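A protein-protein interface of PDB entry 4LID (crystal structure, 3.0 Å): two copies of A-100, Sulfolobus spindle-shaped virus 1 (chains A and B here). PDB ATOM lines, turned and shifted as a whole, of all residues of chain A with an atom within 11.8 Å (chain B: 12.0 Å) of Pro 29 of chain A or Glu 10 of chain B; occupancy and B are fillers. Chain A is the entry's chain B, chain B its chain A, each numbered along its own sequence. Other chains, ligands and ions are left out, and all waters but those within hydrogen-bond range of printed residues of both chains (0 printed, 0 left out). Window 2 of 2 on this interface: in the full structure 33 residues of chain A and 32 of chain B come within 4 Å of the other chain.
The side-chain amino group (NZ) of Lys 28 of chain A is in salt-bridge range of the side-chain carboxylate (OE1) of Glu 11 of chain B. The backbone NH (N) of Arg 27 of chain A lies within hydrogen-bond range of the backbone carbonyl oxygen (O) of Leu 12 of chain B (2.7 Å). The backbone NH (N) of Glu 14 of chain B lies within hydrogen-bond range of the backbone carbonyl oxygen (O) of Leu 25 of chain A (2.8 Å). The side-chain carboxylate (OE1) of Glu 14 of chain B lies within salt-bridge range of the guanidinium group (NH1) of Arg 27 of chain A (3.6 Å). The side-chain carboxylate (OE2) of Glu 14 of chain B sits at hydrogen-bond distance from the side-chain hydroxyl (OG) of Ser 32 of chain A, at 3.1 Å.
O of Gly 26 of chain A lies within hydrogen-bond range of N of Tyr 33 of chain A (2.8 Å). NZ of Lys 28 of chain A lies within salt-bridge range of OE2 of Glu 49 of chain A (3.0 Å). N of Ala 52 of chain A lies within hydrogen-bond range of O of Ser 32 of chain A. The backbone NH (N) of Ser 32 of chain A lies within hydrogen-bond range of the side-chain carboxylate (OD2) of Asp 53 of chain A.
Among the printed residues, merely in contact across the chains: Gly 26 of chain A with Leu 12 of chain B, Arg 27 of chain A with Glu 11 of chain B, His 35 of chain A with Glu 11 of chain B, Pro 29 of chain A with Glu 10 of chain B and Leu 25 of chain A with Leu 13 of chain B.
Of chain B, only Glu 10 comes within 4 Å of Pro 29 of chain A. Glu 10 of chain B touches just one residue of chain A: Pro 29. Of chain B, only Glu 11 comes within 4 Å of Lys 28 of chain A. No residue of chain B comes within 4 Å of Tyr 30 of chain A. No residue of chain B comes within 4 Å of Gly 31 of chain A. Glu 11 of chain B touches three residues of chain A. Printed residues of chain B within 4 Å of His 35 of chain A: Glu 11. Printed residues of chain B within 4 Å of Gly 26 of chain A: Leu 12 (3.3 Å). The nearest residue of chain A that does not touch Glu 10 of chain B is Lys 28 of chain A (4.7 Å). The nearest printed residue of chain B that does not touch Ser 32 of chain A is Leu 12 of chain B (7.2 Å).
Hydrophobic or aromatic side chains of chain A that line the printed part of chain B: Leu 25, Pro 29 and His 35. Among the printed residues, 10 pairs touch across the chains. Among the printed residues, Asp or Glu carboxylates within 4 Å of a Lys or Arg side-chain nitrogen of the other chain: Arg 27 of chain A with Glu 14 of chain B and Lys 28 of chain A with Glu 11 of chain B.
No position is printed for both chains.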
ATOM      1  N   LEU A  25     -28.890   1.102  12.746  1.00  0.00           N
ATOM      2  CA  LEU A  25     -28.503   2.459  12.514  1.00  0.00           C
ATOM      3  C   LEU A  25     -26.977   2.600  12.744  1.00  0.00           C
ATOM      4  O   LEU A  25     -26.498   2.412  13.851  1.00  0.00           O
ATOM      5  CB  LEU A  25     -29.283   3.338  13.454  1.00  0.00           C
ATOM      6  CG  LEU A  25     -29.090   4.831  13.278  1.00  0.00           C
ATOM      7  CD1 LEU A  25     -29.420   5.294  11.863  1.00  0.00           C
ATOM      8  CD2 LEU A  25     -29.975   5.514  14.303  1.00  0.00           C
ATOM      9  N   GLY A  26     -26.215   2.873  11.685  1.00  0.00           N
ATOM     10  CA  GLY A  26     -24.793   3.238  11.795  1.00  0.00           C
ATOM     11  C   GLY A  26     -24.591   4.736  11.620  1.00  0.00           C
ATOM     12  O   GLY A  26     -25.296   5.372  10.842  1.00  0.00           O
ATOM     13  N   ARG A  27     -23.659   5.325  12.369  1.00  0.00           N
ATOM     14  CA  ARG A  27     -23.305   6.725  12.136  1.00  0.00           C
ATOM     15  C   ARG A  27     -21.990   6.802  11.409  1.00  0.00           C
ATOM     16  O   ARG A  27     -21.011   6.222  11.809  1.00  0.00           O
ATOM     17  CB  ARG A  27     -23.235   7.568  13.396  1.00  0.00           C
ATOM     18  CG  ARG A  27     -23.310   9.063  13.071  1.00  0.00           C
ATOM     19  CD  ARG A  27     -23.325   9.968  14.301  1.00  0.00           C
ATOM     20  NE  ARG A  27     -22.072   9.856  15.056  1.00  0.00           N
ATOM     21  CZ  ARG A  27     -21.870   9.073  16.118  1.00  0.00           C
ATOM     22  NH1 ARG A  27     -22.847   8.310  16.594  1.00  0.00           N
ATOM     23  NH2 ARG A  27     -20.679   9.055  16.717  1.00  0.00           N
ATOM     24  N   LYS A  28     -22.032   7.520  10.301  1.00  0.00           N
ATOM     25  CA  LYS A  28     -20.887   7.836   9.477  1.00  0.00           C
ATOM     26  C   LYS A  28     -20.570   9.331   9.683  1.00  0.00           C
ATOM     27  O   LYS A  28     -21.433  10.098  10.196  1.00  0.00           O
ATOM     28  CB  LYS A  28     -21.254   7.564   8.013  1.00  0.00           C
ATOM     29  CG  LYS A  28     -21.109   6.112   7.628  1.00  0.00           C
ATOM     30  CD  LYS A  28     -21.735   5.799   6.289  1.00  0.00           C
ATOM     31  CE  LYS A  28     -21.113   4.560   5.666  1.00  0.00           C
ATOM     32  NZ  LYS A  28     -22.131   3.670   5.033  1.00  0.00           N
ATOM     33  N   PRO A  29     -19.361   9.766   9.243  1.00  0.00           N
ATOM     34  CA  PRO A  29     -18.989  11.200   9.323  1.00  0.00           C
ATOM     35  C   PRO A  29     -20.048  12.174   8.749  1.00  0.00           C
ATOM     36  O   PRO A  29     -20.143  13.298   9.212  1.00  0.00           O
ATOM     37  CB  PRO A  29     -17.690  11.266   8.521  1.00  0.00           C
ATOM     38  CG  PRO A  29     -17.130   9.873   8.562  1.00  0.00           C
ATOM     39  CD  PRO A  29     -18.315   8.959   8.574  1.00  0.00           C
ATOM     40  N   TYR A  30     -20.868  11.716   7.799  1.00  0.00           N
ATOM     41  CA  TYR A  30     -21.824  12.560   7.047  1.00  0.00           C
ATOM     42  C   TYR A  30     -23.253  12.586   7.596  1.00  0.00           C
ATOM     43  O   TYR A  30     -23.992  13.534   7.393  1.00  0.00           O
ATOM     44  CB  TYR A  30     -21.886  12.047   5.612  1.00  0.00           C
ATOM     45  CG  TYR A  30     -20.514  11.865   4.989  1.00  0.00           C
ATOM     46  CD1 TYR A  30     -19.855  12.960   4.394  1.00  0.00           C
ATOM     47  CD2 TYR A  30     -19.864  10.606   5.004  1.00  0.00           C
ATOM     48  CE1 TYR A  30     -18.606  12.816   3.823  1.00  0.00           C
ATOM     49  CE2 TYR A  30     -18.609  10.455   4.436  1.00  0.00           C
ATOM     50  CZ  TYR A  30     -17.989  11.565   3.847  1.00  0.00           C
ATOM     51  OH  TYR A  30     -16.746  11.444   3.273  1.00  0.00           O
ATOM     52  N   GLY A  31     -23.656  11.506   8.251  1.00  0.00           N
ATOM     53  CA  GLY A  31     -24.954  11.428   8.904  1.00  0.00           C
ATOM     54  C   GLY A  31     -25.177   9.984   9.285  1.00  0.00           C
ATOM     55  O   GLY A  31     -24.312   9.135   9.059  1.00  0.00           O
ATOM     56  N   SER A  32     -26.343   9.698   9.843  1.00  0.00           N
ATOM     57  CA  SER A  32     -26.713   8.345  10.157  1.00  0.00           C
ATOM     58  C   SER A  32     -27.309   7.552   8.943  1.00  0.00           C
ATOM     59  O   SER A  32     -27.972   8.107   8.089  1.00  0.00           O
ATOM     60  CB  SER A  32     -27.642   8.397  11.347  1.00  0.00           C
ATOM     61  OG  SER A  32     -26.953   8.953  12.465  1.00  0.00           O
ATOM     62  N   TYR A  33     -26.988   6.263   8.851  1.00  0.00           N
ATOM     63  CA  TYR A  33     -27.414   5.390   7.760  1.00  0.00           C
ATOM     64  C   TYR A  33     -28.119   4.202   8.358  1.00  0.00           C
ATOM     65  O   TYR A  33     -27.733   3.733   9.411  1.00  0.00           O
ATOM     66  CB  TYR A  33     -26.225   4.920   6.913  1.00  0.00           C
ATOM     67  CG  TYR A  33     -25.695   6.061   6.083  1.00  0.00           C
ATOM     68  CD1 TYR A  33     -25.877   6.115   4.698  1.00  0.00           C
ATOM     69  CD2 TYR A  33     -25.083   7.147   6.703  1.00  0.00           C
ATOM     70  CE1 TYR A  33     -25.424   7.205   3.970  1.00  0.00           C
ATOM     71  CE2 TYR A  33     -24.621   8.230   5.987  1.00  0.00           C
ATOM     72  CZ  TYR A  33     -24.788   8.253   4.632  1.00  0.00           C
ATOM     73  OH  TYR A  33     -24.310   9.352   3.981  1.00  0.00           O
ATOM     74  N   LEU A  34     -29.159   3.724   7.687  1.00  0.00           N
ATOM     75  CA  LEU A  34     -30.037   2.687   8.219  1.00  0.00           C
ATOM     76  C   LEU A  34     -29.872   1.486   7.331  1.00  0.00           C
ATOM     77  O   LEU A  34     -30.206   1.533   6.149  1.00  0.00           O
ATOM     78  CB  LEU A  34     -31.465   3.162   8.213  1.00  0.00           C
ATOM     79  CG  LEU A  34     -32.555   2.203   8.690  1.00  0.00           C
ATOM     80  CD1 LEU A  34     -32.594   0.902   7.888  1.00  0.00           C
ATOM     81  CD2 LEU A  34     -32.299   1.853  10.143  1.00  0.00           C
ATOM     82  N   HIS A  35     -29.283   0.432   7.884  1.00  0.00           N
ATOM     83  CA  HIS A  35     -29.050  -0.768   7.141  1.00  0.00           C
ATOM     84  C   HIS A  35     -30.270  -1.593   7.420  1.00  0.00           C
ATOM     85  O   HIS A  35     -30.666  -1.837   8.558  1.00  0.00           O
ATOM     86  CB  HIS A  35     -27.785  -1.467   7.560  1.00  0.00           C
ATOM     87  CG  HIS A  35     -26.586  -0.574   7.568  1.00  0.00           C
ATOM     88  ND1 HIS A  35     -25.627  -0.599   6.580  1.00  0.00           N
ATOM     89  CD2 HIS A  35     -26.187   0.375   8.453  1.00  0.00           C
ATOM     90  CE1 HIS A  35     -24.687   0.291   6.857  1.00  0.00           C
ATOM     91  NE2 HIS A  35     -24.999   0.890   7.994  1.00  0.00           N
ATOM     92  N   GLU A  49     -29.338   0.189   2.206  1.00  0.00           N
ATOM     93  CA  GLU A  49     -28.727   1.104   3.113  1.00  0.00           C
ATOM     94  C   GLU A  49     -29.243   2.470   2.720  1.00  0.00           C
ATOM     95  O   GLU A  49     -28.859   3.000   1.706  1.00  0.00           O
ATOM     96  CB  GLU A  49     -27.222   1.021   2.967  1.00  0.00           C
ATOM     97  CG  GLU A  49     -26.477   1.234   4.261  1.00  0.00           C
ATOM     98  CD  GLU A  49     -25.123   1.892   4.059  1.00  0.00           C
ATOM     99  OE1 GLU A  49     -24.207   1.243   3.511  1.00  0.00           O
ATOM    100  OE2 GLU A  49     -24.973   3.068   4.453  1.00  0.00           O
ATOM    101  N   TYR A  51     -29.997   6.558   3.801  1.00  0.00           N
ATOM    102  CA  TYR A  51     -29.535   7.649   4.639  1.00  0.00           C
ATOM    103  C   TYR A  51     -30.714   7.910   5.551  1.00  0.00           C
ATOM    104  O   TYR A  51     -31.807   8.131   5.095  1.00  0.00           O
ATOM    105  CB  TYR A  51     -29.171   8.853   3.755  1.00  0.00           C
ATOM    106  CG  TYR A  51     -28.881  10.116   4.480  1.00  0.00           C
ATOM    107  CD1 TYR A  51     -27.609  10.402   4.939  1.00  0.00           C
ATOM    108  CD2 TYR A  51     -29.877  11.046   4.686  1.00  0.00           C
ATOM    109  CE1 TYR A  51     -27.343  11.583   5.609  1.00  0.00           C
ATOM    110  CE2 TYR A  51     -29.627  12.229   5.348  1.00  0.00           C
ATOM    111  CZ  TYR A  51     -28.364  12.485   5.817  1.00  0.00           C
ATOM    112  OH  TYR A  51     -28.144  13.650   6.484  1.00  0.00           O
ATOM    113  N   ALA A  52     -30.508   7.862   6.836  1.00  0.00           N
ATOM    114  CA  ALA A  52     -31.629   7.812   7.781  1.00  0.00           C
ATOM    115  C   ALA A  52     -32.250   9.150   8.106  1.00  0.00           C
ATOM    116  O   ALA A  52     -33.429   9.197   8.488  1.00  0.00           O
ATOM    117  CB  ALA A  52     -31.186   7.161   9.082  1.00  0.00           C
ATOM    118  N   ASP A  53     -31.469  10.224   7.977  1.00  0.00           N
ATOM    119  CA  ASP A  53     -31.831  11.505   8.590  1.00  0.00           C
ATOM    120  C   ASP A  53     -33.030  12.196   7.930  1.00  0.00           C
ATOM    121  O   ASP A  53     -33.633  13.051   8.535  1.00  0.00           O
ATOM    122  CB  ASP A  53     -30.626  12.451   8.623  1.00  0.00           C
ATOM    123  CG  ASP A  53     -29.547  12.020   9.625  1.00  0.00           C
ATOM    124  OD1 ASP A  53     -29.890  11.828  10.821  1.00  0.00           O
ATOM    125  OD2 ASP A  53     -28.360  11.913   9.214  1.00  0.00           O
ATOM    126  N   GLU B  10     -15.050   2.610   9.500  1.00  0.00           N
ATOM    127  CA  GLU B  10     -15.297   3.952   8.982  1.00  0.00           C
ATOM    128  C   GLU B  10     -16.579   4.509   9.550  1.00  0.00           C
ATOM    129  O   GLU B  10     -16.747   5.716   9.644  1.00  0.00           O
ATOM    130  CB  GLU B  10     -15.396   3.920   7.462  1.00  0.00           C
ATOM    131  CG  GLU B  10     -15.575   5.290   6.836  1.00  0.00           C
ATOM    132  CD  GLU B  10     -15.615   5.234   5.325  1.00  0.00           C
ATOM    133  OE1 GLU B  10     -15.561   4.118   4.769  1.00  0.00           O
ATOM    134  OE2 GLU B  10     -15.700   6.309   4.699  1.00  0.00           O
ATOM    135  N   GLU B  11     -17.479   3.609   9.930  1.00  0.00           N
ATOM    136  CA  GLU B  11     -18.762   3.979  10.493  1.00  0.00           C
ATOM    137  C   GLU B  11     -19.012   3.203  11.755  1.00  0.00           C
ATOM    138  O   GLU B  11     -18.475   2.139  11.935  1.00  0.00           O
ATOM    139  CB  GLU B  11     -19.856   3.634   9.525  1.00  0.00           C
ATOM    140  CG  GLU B  11     -19.951   2.153   9.278  1.00  0.00           C
ATOM    141  CD  GLU B  11     -20.968   1.822   8.225  1.00  0.00           C
ATOM    142  OE1 GLU B  11     -21.849   2.660   7.973  1.00  0.00           O
ATOM    143  OE2 GLU B  11     -20.874   0.724   7.645  1.00  0.00           O
ATOM    144  N   LEU B  12     -19.845   3.734  12.627  1.00  0.00           N
ATOM    145  CA  LEU B  12     -20.038   3.147  13.937  1.00  0.00           C
ATOM    146  C   LEU B  12     -21.483   2.793  14.206  1.00  0.00           C
ATOM    147  O   LEU B  12     -22.350   3.596  13.987  1.00  0.00           O
ATOM    148  CB  LEU B  12     -19.569   4.139  14.985  1.00  0.00           C
ATOM    149  CG  LEU B  12     -19.370   3.610  16.394  1.00  0.00           C
ATOM    150  CD1 LEU B  12     -17.910   3.351  16.623  1.00  0.00           C
ATOM    151  CD2 LEU B  12     -19.892   4.603  17.409  1.00  0.00           C
ATOM    152  N   LEU B  13     -21.732   1.591  14.698  1.00  0.00           N
ATOM    153  CA  LEU B  13     -23.083   1.110  14.928  1.00  0.00           C
ATOM    154  C   LEU B  13     -23.607   1.713  16.175  1.00  0.00           C
ATOM    155  O   LEU B  13     -22.901   1.842  17.160  1.00  0.00           O
ATOM    156  CB  LEU B  13     -23.147  -0.396  15.041  1.00  0.00           C
ATOM    157  CG  LEU B  13     -22.642  -1.049  13.734  1.00  0.00           C
ATOM    158  CD1 LEU B  13     -23.228  -2.445  13.694  1.00  0.00           C
ATOM    159  CD2 LEU B  13     -22.921  -0.308  12.397  1.00  0.00           C
ATOM    160  N   GLU B  14     -24.834   2.176  16.107  1.00  0.00           N
ATOM    161  CA  GLU B  14     -25.365   2.901  17.203  1.00  0.00           C
ATOM    162  C   GLU B  14     -26.353   2.011  17.894  1.00  0.00           C
ATOM    163  O   GLU B  14     -26.383   1.955  19.102  1.00  0.00           O
ATOM    164  CB  GLU B  14     -26.041   4.162  16.725  1.00  0.00           C
ATOM    165  CG  GLU B  14     -25.139   5.231  16.133  1.00  0.00           C
ATOM    166  CD  GLU B  14     -25.944   6.494  15.831  1.00  0.00           C
ATOM    167  OE1 GLU B  14     -26.293   7.193  16.806  1.00  0.00           O
ATOM    168  OE2 GLU B  14     -26.254   6.788  14.641  1.00  0.00           O
